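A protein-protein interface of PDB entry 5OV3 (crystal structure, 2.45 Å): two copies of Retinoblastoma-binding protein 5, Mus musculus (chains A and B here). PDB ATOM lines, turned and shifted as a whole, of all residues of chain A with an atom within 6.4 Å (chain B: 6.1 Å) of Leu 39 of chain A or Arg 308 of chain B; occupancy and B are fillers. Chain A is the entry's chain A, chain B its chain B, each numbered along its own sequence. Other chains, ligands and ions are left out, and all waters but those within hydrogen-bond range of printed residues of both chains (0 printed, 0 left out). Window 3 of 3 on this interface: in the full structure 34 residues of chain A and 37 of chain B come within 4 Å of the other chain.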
ATOM      1  N   THR A  32     -15.839  41.613   5.422  1.00  0.00           N
ATOM      2  CA  THR A  32     -15.718  41.164   4.034  1.00  0.00           C
ATOM      3  C   THR A  32     -16.332  39.765   3.849  1.00  0.00           C
ATOM      4  O   THR A  32     -16.203  38.889   4.713  1.00  0.00           O
ATOM      5  CB  THR A  32     -14.237  41.194   3.589  1.00  0.00           C
ATOM      6  OG1 THR A  32     -14.095  40.644   2.273  1.00  0.00           O
ATOM      7  CG2 THR A  32     -13.337  40.423   4.539  1.00  0.00           C
ATOM      8  N   PHE A  33     -17.022  39.573   2.727  1.00  0.00           N
ATOM      9  CA  PHE A  33     -17.632  38.289   2.413  1.00  0.00           C
ATOM     10  C   PHE A  33     -16.622  37.318   1.814  1.00  0.00           C
ATOM     11  O   PHE A  33     -15.653  37.707   1.151  1.00  0.00           O
ATOM     12  CB  PHE A  33     -18.762  38.439   1.398  1.00  0.00           C
ATOM     13  CG  PHE A  33     -19.911  39.268   1.877  1.00  0.00           C
ATOM     14  CD1 PHE A  33     -20.961  38.677   2.558  1.00  0.00           C
ATOM     15  CD2 PHE A  33     -19.946  40.640   1.633  1.00  0.00           C
ATOM     16  CE1 PHE A  33     -22.037  39.423   2.998  1.00  0.00           C
ATOM     17  CE2 PHE A  33     -21.014  41.401   2.067  1.00  0.00           C
ATOM     18  CZ  PHE A  33     -22.079  40.782   2.752  1.00  0.00           C
ATOM     19  N   ASN A  34     -16.879  36.031   2.013  1.00  0.00           N
ATOM     20  CA  ASN A  34     -16.108  35.094   1.217  1.00  0.00           C
ATOM     21  C   ASN A  34     -16.671  35.056  -0.204  1.00  0.00           C
ATOM     22  O   ASN A  34     -17.673  35.695  -0.527  1.00  0.00           O
ATOM     23  CB  ASN A  34     -16.042  33.708   1.883  1.00  0.00           C
ATOM     24  CG  ASN A  34     -17.404  32.940   1.913  1.00  0.00           C
ATOM     25  OD1 ASN A  34     -18.485  33.485   1.675  1.00  0.00           O
ATOM     26  ND2 ASN A  34     -17.319  31.659   2.239  1.00  0.00           N
ATOM     27  N   ARG A  35     -15.994  34.313  -1.070  1.00  0.00           N
ATOM     28  CA  ARG A  35     -16.298  34.402  -2.494  1.00  0.00           C
ATOM     29  C   ARG A  35     -17.732  33.958  -2.804  1.00  0.00           C
ATOM     30  O   ARG A  35     -18.354  34.489  -3.729  1.00  0.00           O
ATOM     31  CB  ARG A  35     -15.232  33.615  -3.272  1.00  0.00           C
ATOM     32  CG  ARG A  35     -15.660  32.861  -4.522  1.00  0.00           C
ATOM     33  CD  ARG A  35     -14.485  32.040  -5.073  1.00  0.00           C
ATOM     34  NE  ARG A  35     -14.805  31.387  -6.341  1.00  0.00           N
ATOM     35  CZ  ARG A  35     -14.576  31.915  -7.537  1.00  0.00           C
ATOM     36  NH1 ARG A  35     -14.030  33.119  -7.617  1.00  0.00           N
ATOM     37  NH2 ARG A  35     -14.897  31.243  -8.635  1.00  0.00           N
ATOM     38  N   TRP A  36     -18.307  33.056  -2.000  1.00  0.00           N
ATOM     39  CA  TRP A  36     -19.696  32.642  -2.203  1.00  0.00           C
ATOM     40  C   TRP A  36     -20.698  33.397  -1.336  1.00  0.00           C
ATOM     41  O   TRP A  36     -21.905  33.196  -1.502  1.00  0.00           O
ATOM     42  CB  TRP A  36     -19.833  31.128  -1.967  1.00  0.00           C
ATOM     43  CG  TRP A  36     -18.737  30.399  -2.669  1.00  0.00           C
ATOM     44  CD1 TRP A  36     -18.658  30.115  -4.012  1.00  0.00           C
ATOM     45  CD2 TRP A  36     -17.508  29.941  -2.089  1.00  0.00           C
ATOM     46  NE1 TRP A  36     -17.468  29.480  -4.293  1.00  0.00           N
ATOM     47  CE2 TRP A  36     -16.742  29.363  -3.133  1.00  0.00           C
ATOM     48  CE3 TRP A  36     -16.989  29.944  -0.784  1.00  0.00           C
ATOM     49  CZ2 TRP A  36     -15.484  28.793  -2.909  1.00  0.00           C
ATOM     50  CZ3 TRP A  36     -15.745  29.383  -0.564  1.00  0.00           C
ATOM     51  CH2 TRP A  36     -15.004  28.816  -1.622  1.00  0.00           C
ATOM     52  N   GLY A  37     -20.245  34.268  -0.437  1.00  0.00           N
ATOM     53  CA  GLY A  37     -21.179  34.987   0.407  1.00  0.00           C
ATOM     54  C   GLY A  37     -21.989  34.089   1.317  1.00  0.00           C
ATOM     55  O   GLY A  37     -23.152  34.378   1.591  1.00  0.00           O
ATOM     56  N   THR A  38     -21.411  32.982   1.758  1.00  0.00           N
ATOM     57  CA  THR A  38     -21.960  32.195   2.851  1.00  0.00           C
ATOM     58  C   THR A  38     -21.430  32.641   4.198  1.00  0.00           C
ATOM     59  O   THR A  38     -22.079  32.399   5.221  1.00  0.00           O
ATOM     60  CB  THR A  38     -21.621  30.717   2.652  1.00  0.00           C
ATOM     61  OG1 THR A  38     -20.246  30.613   2.240  1.00  0.00           O
ATOM     62  CG2 THR A  38     -22.510  30.124   1.580  1.00  0.00           C
ATOM     63  N   LEU A  39     -20.271  33.295   4.219  1.00  0.00           N
ATOM     64  CA  LEU A  39     -19.641  33.708   5.457  1.00  0.00           C
ATOM     65  C   LEU A  39     -19.253  35.180   5.364  1.00  0.00           C
ATOM     66  O   LEU A  39     -18.902  35.689   4.292  1.00  0.00           O
ATOM     67  CB  LEU A  39     -18.413  32.829   5.757  1.00  0.00           C
ATOM     68  CG  LEU A  39     -18.660  31.314   5.774  1.00  0.00           C
ATOM     69  CD1 LEU A  39     -17.338  30.570   5.789  1.00  0.00           C
ATOM     70  CD2 LEU A  39     -19.525  30.920   6.968  1.00  0.00           C
ATOM     71  N   LEU A  40     -19.320  35.853   6.507  1.00  0.00           N
ATOM     72  CA  LEU A  40     -18.934  37.249   6.647  1.00  0.00           C
ATOM     73  C   LEU A  40     -17.844  37.343   7.711  1.00  0.00           C
ATOM     74  O   LEU A  40     -18.113  37.171   8.906  1.00  0.00           O
ATOM     75  CB  LEU A  40     -20.139  38.108   7.022  1.00  0.00           C
ATOM     76  CG  LEU A  40     -19.845  39.617   6.985  1.00  0.00           C
ATOM     77  CD1 LEU A  40     -19.583  40.041   5.552  1.00  0.00           C
ATOM     78  CD2 LEU A  40     -20.994  40.424   7.559  1.00  0.00           C
ATOM     79  N   ALA A  41     -16.616  37.614   7.282  1.00  0.00           N
ATOM     80  CA  ALA A  41     -15.523  37.840   8.219  1.00  0.00           C
ATOM     81  C   ALA A  41     -15.618  39.259   8.771  1.00  0.00           C
ATOM     82  O   ALA A  41     -15.670  40.223   8.001  1.00  0.00           O
ATOM     83  CB  ALA A  41     -14.187  37.598   7.526  1.00  0.00           C
ATOM     84  N   ILE A  51     -16.404  35.197  12.461  1.00  0.00           N
ATOM     85  CA  ILE A  51     -16.941  34.814  11.166  1.00  0.00           C
ATOM     86  C   ILE A  51     -18.394  34.419  11.346  1.00  0.00           C
ATOM     87  O   ILE A  51     -18.704  33.423  12.013  1.00  0.00           O
ATOM     88  CB  ILE A  51     -16.137  33.685  10.515  1.00  0.00           C
ATOM     89  CG1 ILE A  51     -14.652  34.048  10.524  1.00  0.00           C
ATOM     90  CG2 ILE A  51     -16.641  33.471   9.098  1.00  0.00           C
ATOM     91  CD1 ILE A  51     -13.848  33.348   9.460  1.00  0.00           C
ATOM     92  N   TRP A  52     -19.279  35.195  10.742  1.00  0.00           N
ATOM     93  CA  TRP A  52     -20.709  34.982  10.848  1.00  0.00           C
ATOM     94  C   TRP A  52     -21.207  34.178   9.650  1.00  0.00           C
ATOM     95  O   TRP A  52     -20.756  34.380   8.518  1.00  0.00           O
ATOM     96  CB  TRP A  52     -21.432  36.327  10.951  1.00  0.00           C
ATOM     97  CG  TRP A  52     -22.870  36.213  11.335  1.00  0.00           C
ATOM     98  CD1 TRP A  52     -23.379  36.005  12.590  1.00  0.00           C
ATOM     99  CD2 TRP A  52     -23.996  36.329  10.462  1.00  0.00           C
ATOM    100  NE1 TRP A  52     -24.755  35.974  12.546  1.00  0.00           N
ATOM    101  CE2 TRP A  52     -25.156  36.185  11.251  1.00  0.00           C
ATOM    102  CE3 TRP A  52     -24.136  36.561   9.088  1.00  0.00           C
ATOM    103  CZ2 TRP A  52     -26.438  36.262  10.713  1.00  0.00           C
ATOM    104  CZ3 TRP A  52     -25.421  36.635   8.556  1.00  0.00           C
ATOM    105  CH2 TRP A  52     -26.552  36.483   9.370  1.00  0.00           C
ATOM    106  N   ASP A  53     -22.143  33.274   9.908  1.00  0.00           N
ATOM    107  CA  ASP A  53     -22.633  32.311   8.926  1.00  0.00           C
ATOM    108  C   ASP A  53     -24.022  32.736   8.453  1.00  0.00           C
ATOM    109  O   ASP A  53     -24.946  32.879   9.258  1.00  0.00           O
ATOM    110  CB  ASP A  53     -22.641  30.908   9.545  1.00  0.00           C
ATOM    111  CG  ASP A  53     -23.184  29.824   8.606  1.00  0.00           C
ATOM    112  OD1 ASP A  53     -22.934  29.838   7.382  1.00  0.00           O
ATOM    113  OD2 ASP A  53     -23.873  28.921   9.121  1.00  0.00           O
ATOM    114  N   PHE A  54     -24.155  32.968   7.152  1.00  0.00           N
ATOM    115  CA  PHE A  54     -25.450  33.300   6.581  1.00  0.00           C
ATOM    116  C   PHE A  54     -26.421  32.116   6.582  1.00  0.00           C
ATOM    117  O   PHE A  54     -27.634  32.330   6.512  1.00  0.00           O
ATOM    118  CB  PHE A  54     -25.267  33.818   5.159  1.00  0.00           C
ATOM    119  CG  PHE A  54     -25.113  35.321   5.074  1.00  0.00           C
ATOM    120  CD1 PHE A  54     -23.952  35.934   5.491  1.00  0.00           C
ATOM    121  CD2 PHE A  54     -26.130  36.107   4.567  1.00  0.00           C
ATOM    122  CE1 PHE A  54     -23.817  37.306   5.423  1.00  0.00           C
ATOM    123  CE2 PHE A  54     -26.006  37.474   4.492  1.00  0.00           C
ATOM    124  CZ  PHE A  54     -24.845  38.081   4.922  1.00  0.00           C
ATOM    125  N   LEU A  55     -25.930  30.881   6.665  1.00  0.00           N
ATOM    126  CA  LEU A  55     -26.845  29.744   6.607  1.00  0.00           C
ATOM    127  C   LEU A  55     -27.494  29.485   7.963  1.00  0.00           C
ATOM    128  O   LEU A  55     -28.723  29.480   8.068  1.00  0.00           O
ATOM    129  CB  LEU A  55     -26.119  28.504   6.089  1.00  0.00           C
ATOM    130  CG  LEU A  55     -25.517  28.716   4.697  1.00  0.00           C
ATOM    131  CD1 LEU A  55     -24.887  27.456   4.170  1.00  0.00           C
ATOM    132  CD2 LEU A  55     -26.569  29.204   3.750  1.00  0.00           C
ATOM    133  N   THR A  56     -26.689  29.326   9.019  1.00  0.00           N
ATOM    134  CA  THR A  56     -27.250  29.160  10.358  1.00  0.00           C
ATOM    135  C   THR A  56     -27.662  30.469  11.012  1.00  0.00           C
ATOM    136  O   THR A  56     -28.225  30.428  12.110  1.00  0.00           O
ATOM    137  CB  THR A  56     -26.262  28.493  11.313  1.00  0.00           C
ATOM    138  OG1 THR A  56     -25.130  29.361  11.504  1.00  0.00           O
ATOM    139  CG2 THR A  56     -25.821  27.139  10.783  1.00  0.00           C
ATOM    140  N   ALA A  60     -19.771  31.226  12.876  1.00  0.00           N
ATOM    141  CA  ALA A  60     -19.104  30.040  12.367  1.00  0.00           C
ATOM    142  C   ALA A  60     -17.743  29.819  13.004  1.00  0.00           C
ATOM    143  O   ALA A  60     -17.339  28.669  13.200  1.00  0.00           O
ATOM    144  CB  ALA A  60     -18.928  30.138  10.849  1.00  0.00           C
ATOM    145  N   TRP A  75     -10.273  37.572   2.077  1.00  0.00           N
ATOM    146  CA  TRP A  75     -10.415  36.122   1.943  1.00  0.00           C
ATOM    147  C   TRP A  75      -9.582  35.622   0.770  1.00  0.00           C
ATOM    148  O   TRP A  75      -9.609  36.213  -0.316  1.00  0.00           O
ATOM    149  CB  TRP A  75     -11.869  35.720   1.694  1.00  0.00           C
ATOM    150  CG  TRP A  75     -12.835  35.768   2.833  1.00  0.00           C
ATOM    151  CD1 TRP A  75     -13.649  36.814   3.169  1.00  0.00           C
ATOM    152  CD2 TRP A  75     -13.178  34.694   3.727  1.00  0.00           C
ATOM    153  NE1 TRP A  75     -14.439  36.480   4.247  1.00  0.00           N
ATOM    154  CE2 TRP A  75     -14.184  35.182   4.600  1.00  0.00           C
ATOM    155  CE3 TRP A  75     -12.726  33.382   3.882  1.00  0.00           C
ATOM    156  CZ2 TRP A  75     -14.744  34.401   5.614  1.00  0.00           C
ATOM    157  CZ3 TRP A  75     -13.280  32.606   4.889  1.00  0.00           C
ATOM    158  CH2 TRP A  75     -14.275  33.119   5.747  1.00  0.00           C
ATOM    159  N   GLY A  79     -11.079  30.309  -0.174  1.00  0.00           N
ATOM    160  CA  GLY A  79     -11.952  30.433   0.969  1.00  0.00           C
ATOM    161  C   GLY A  79     -11.429  29.860   2.264  1.00  0.00           C
ATOM    162  O   GLY A  79     -12.144  29.930   3.271  1.00  0.00           O
ATOM    163  N   VAL A  96      -8.895  29.587   8.339  1.00  0.00           N
ATOM    164  CA  VAL A  96     -10.235  29.808   8.880  1.00  0.00           C
ATOM    165  C   VAL A  96     -10.781  28.558   9.559  1.00  0.00           C
ATOM    166  O   VAL A  96     -11.614  28.658  10.467  1.00  0.00           O
ATOM    167  CB  VAL A  96     -11.199  30.294   7.785  1.00  0.00           C
ATOM    168  CG1 VAL A  96     -10.730  31.632   7.234  1.00  0.00           C
ATOM    169  CG2 VAL A  96     -11.332  29.278   6.681  1.00  0.00           C
ATOM    170  N   GLY B 262     -24.855  15.914   6.813  1.00  0.00           N
ATOM    171  CA  GLY B 262     -23.977  16.133   5.673  1.00  0.00           C
ATOM    172  C   GLY B 262     -22.668  15.369   5.766  1.00  0.00           C
ATOM    173  O   GLY B 262     -22.163  14.867   4.764  1.00  0.00           O
ATOM    174  N   TRP B 304     -31.817  16.856   5.714  1.00  0.00           N
ATOM    175  CA  TRP B 304     -30.723  17.408   6.485  1.00  0.00           C
ATOM    176  C   TRP B 304     -29.869  18.248   5.543  1.00  0.00           C
ATOM    177  O   TRP B 304     -29.556  17.814   4.426  1.00  0.00           O
ATOM    178  CB  TRP B 304     -29.912  16.300   7.162  1.00  0.00           C
ATOM    179  CG  TRP B 304     -29.087  16.817   8.312  1.00  0.00           C
ATOM    180  CD1 TRP B 304     -28.249  17.889   8.278  1.00  0.00           C
ATOM    181  CD2 TRP B 304     -29.020  16.306   9.651  1.00  0.00           C
ATOM    182  NE1 TRP B 304     -27.663  18.079   9.503  1.00  0.00           N
ATOM    183  CE2 TRP B 304     -28.110  17.118  10.362  1.00  0.00           C
ATOM    184  CE3 TRP B 304     -29.609  15.230  10.308  1.00  0.00           C
ATOM    185  CZ2 TRP B 304     -27.787  16.895  11.694  1.00  0.00           C
ATOM    186  CZ3 TRP B 304     -29.292  15.017  11.633  1.00  0.00           C
ATOM    187  CH2 TRP B 304     -28.389  15.842  12.310  1.00  0.00           C
ATOM    188  N   HIS B 305     -29.523  19.442   5.988  1.00  0.00           N
ATOM    189  CA  HIS B 305     -28.674  20.349   5.209  1.00  0.00           C
ATOM    190  C   HIS B 305     -27.327  19.715   4.869  1.00  0.00           C
ATOM    191  O   HIS B 305     -26.634  19.218   5.776  1.00  0.00           O
ATOM    192  CB  HIS B 305     -28.459  21.616   6.018  1.00  0.00           C
ATOM    193  CG  HIS B 305     -27.885  22.741   5.230  1.00  0.00           C
ATOM    194  ND1 HIS B 305     -26.580  22.747   4.790  1.00  0.00           N
ATOM    195  CD2 HIS B 305     -28.443  23.894   4.794  1.00  0.00           C
ATOM    196  CE1 HIS B 305     -26.365  23.862   4.114  1.00  0.00           C
ATOM    197  NE2 HIS B 305     -27.480  24.569   4.097  1.00  0.00           N
ATOM    198  N   PRO B 306     -26.887  19.772   3.608  1.00  0.00           N
ATOM    199  CA  PRO B 306     -25.610  19.131   3.219  1.00  0.00           C
ATOM    200  C   PRO B 306     -24.358  19.607   3.964  1.00  0.00           C
ATOM    201  O   PRO B 306     -23.379  18.851   4.012  1.00  0.00           O
ATOM    202  CB  PRO B 306     -25.496  19.451   1.718  1.00  0.00           C
ATOM    203  CG  PRO B 306     -26.382  20.638   1.498  1.00  0.00           C
ATOM    204  CD  PRO B 306     -27.523  20.470   2.482  1.00  0.00           C
ATOM    205  N   VAL B 307     -24.321  20.826   4.520  1.00  0.00           N
ATOM    206  CA  VAL B 307     -23.074  21.293   5.114  1.00  0.00           C
ATOM    207  C   VAL B 307     -23.300  22.047   6.426  1.00  0.00           C
ATOM    208  O   VAL B 307     -22.375  22.683   6.940  1.00  0.00           O
ATOM    209  CB  VAL B 307     -22.269  22.175   4.114  1.00  0.00           C
ATOM    210  CG1 VAL B 307     -21.743  21.350   2.923  1.00  0.00           C
ATOM    211  CG2 VAL B 307     -23.094  23.310   3.567  1.00  0.00           C
ATOM    212  N   ARG B 308     -24.497  22.004   6.989  1.00  0.00           N
ATOM    213  CA  ARG B 308     -24.759  22.740   8.219  1.00  0.00           C
ATOM    214  C   ARG B 308     -25.639  21.935   9.163  1.00  0.00           C
ATOM    215  O   ARG B 308     -26.322  20.990   8.745  1.00  0.00           O
ATOM    216  CB  ARG B 308     -25.436  24.086   7.934  1.00  0.00           C
ATOM    217  CG  ARG B 308     -24.564  25.087   7.208  1.00  0.00           C
ATOM    218  CD  ARG B 308     -23.444  25.594   8.088  1.00  0.00           C
ATOM    219  NE  ARG B 308     -22.877  26.827   7.553  1.00  0.00           N
ATOM    220  CZ  ARG B 308     -21.992  26.872   6.560  1.00  0.00           C
ATOM    221  NH1 ARG B 308     -21.552  25.741   6.025  1.00  0.00           N
ATOM    222  NH2 ARG B 308     -21.532  28.045   6.116  1.00  0.00           N
ATOM    223  N   PRO B 309     -25.650  22.310  10.527  1.00  0.00           N
ATOM    224  CA  PRO B 309     -26.642  21.703  11.438  1.00  0.00           C
ATOM    225  C   PRO B 309     -28.006  22.352  11.252  1.00  0.00           C
ATOM    226  O   PRO B 309     -28.529  23.101  12.092  1.00  0.00           O
ATOM    227  CB  PRO B 309     -26.033  21.970  12.814  1.00  0.00           C
ATOM    228  CG  PRO B 309     -25.216  23.230  12.630  1.00  0.00           C
ATOM    229  CD  PRO B 309     -24.870  23.370  11.186  1.00  0.00           C
ATOM    230  N   ILE B 310     -28.593  22.080  10.095  1.00  0.00           N
ATOM    231  CA  ILE B 310     -29.914  22.586   9.749  1.00  0.00           C
ATOM    232  C   ILE B 310     -30.766  21.438   9.224  1.00  0.00           C
ATOM    233  O   ILE B 310     -30.313  20.626   8.405  1.00  0.00           O
ATOM    234  CB  ILE B 310     -29.825  23.724   8.710  1.00  0.00           C
ATOM    235  CG1 ILE B 310     -29.161  24.962   9.325  1.00  0.00           C
ATOM    236  CG2 ILE B 310     -31.207  24.071   8.166  1.00  0.00           C
ATOM    237  CD1 ILE B 310     -28.627  25.897   8.282  1.00  0.00           C
ATOM    238  N   ILE B 311     -32.009  21.378   9.691  1.00  0.00           N
ATOM    239  CA  ILE B 311     -32.987  20.427   9.184  1.00  0.00           C
ATOM    240  C   ILE B 311     -34.198  21.203   8.677  1.00  0.00           C
ATOM    241  O   ILE B 311     -34.726  22.072   9.377  1.00  0.00           O
ATOM    242  CB  ILE B 311     -33.366  19.406  10.274  1.00  0.00           C
ATOM    243  CG1 ILE B 311     -32.078  18.779  10.822  1.00  0.00           C
ATOM    244  CG2 ILE B 311     -34.310  18.360   9.722  1.00  0.00           C
ATOM    245  CD1 ILE B 311     -32.256  17.701  11.787  1.00  0.00           C
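The backbone NH (N) of Asn 34 of chain A lies within hydrogen-bond range of the backbone carbonyl oxygen (O) of Leu 39 of chain A (3.1 Å). The backbone NH of Leu 55 of chain A lies close to the side-chain carboxylate of Asp 53 of chain A (3.3 Å). OD2 of Asp 53 of chain A lies within hydrogen-bond range of OG1 of Thr 56 of chain A (2.7 Å). A ring nitrogen (ND1) of His 305 of chain B sits at hydrogen-bond distance from the backbone NH of Val 307 of chain B. A ring nitrogen (ND1) of His 305 of chain B is in hydrogen-bond range of the backbone NH of Arg 308 of chain B. O of Ile 310 of chain B lies within hydrogen-bond range of N of His 305 of chain B, 2.8 Å away.
No position is printed for both chains. Of the 8 pairs that touch across the chains among the printed residues, none has its exchanged pair printed and touching as well.
Leu 39 of chain A touches one residue of chain B. Of the printed residues of chain B, Asp 53 of chain A touches Arg 308. Of the printed residues of chain B, Leu 55 of chain A touches His 305, Arg 308 and Ile 310. Of the printed residues of chain A, His 305 of chain B touches Leu 55 (3.9 Å). Printed residues of chain A within 4 Å of Arg 308 of chain B: Leu 39 (3.6 Å), Asp 53 (2.6 Å), Leu 55 (3.8 Å) and Thr 56 (3.9 Å). Of the printed residues of chain A, Ile 310 of chain B touches Leu 55 (3.6 Å) and Thr 56 (3.96 Å). The nearest printed residue of chain B that does not touch Leu 39 of chain A is Val 307 of chain B (8.7 Å). The nearest printed residue of chain B that does not touch Asp 53 of chain A is Ile 310 of chain B (5.7 Å).
NH2 of Arg 308 of chain B lies within salt-bridge range of OD1 of Asp 53 of chain A.
NH2 of Arg 308 of chain B touches CD2 of Leu 39 of chain A (3.6 Å). Leu 55 of chain A touches His 305 of chain B. Arg 308 of chain B touches Leu 55 of chain A (CZ to CD1, 3.8 Å). Ile 310 of chain B touches Leu 55 of chain A. Thr 56 of chain A touches Arg 308 of chain B (CG2 to CD, 3.9 Å). Pro 309 of chain B touches Thr 56 of chain A (CD to CG2, 3.9 Å). Ile 310 of chain B touches Thr 56 of chain A (CD1 to CG2, 3.96 Å).
Printed residues of chain B that touch a printed residue of chain A: His 305, Arg 308, Pro 309 and Ile 310. Hydrophobic or aromatic side chains of chain A within 4 Å of the printed part of chain B: Leu 39 and Leu 55. Among the printed residues, Asp or Glu carboxylates within 4 Å of a Lys or Arg side-chain nitrogen of the other chain: Asp 53 of chain A with Arg 308 of chain B.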
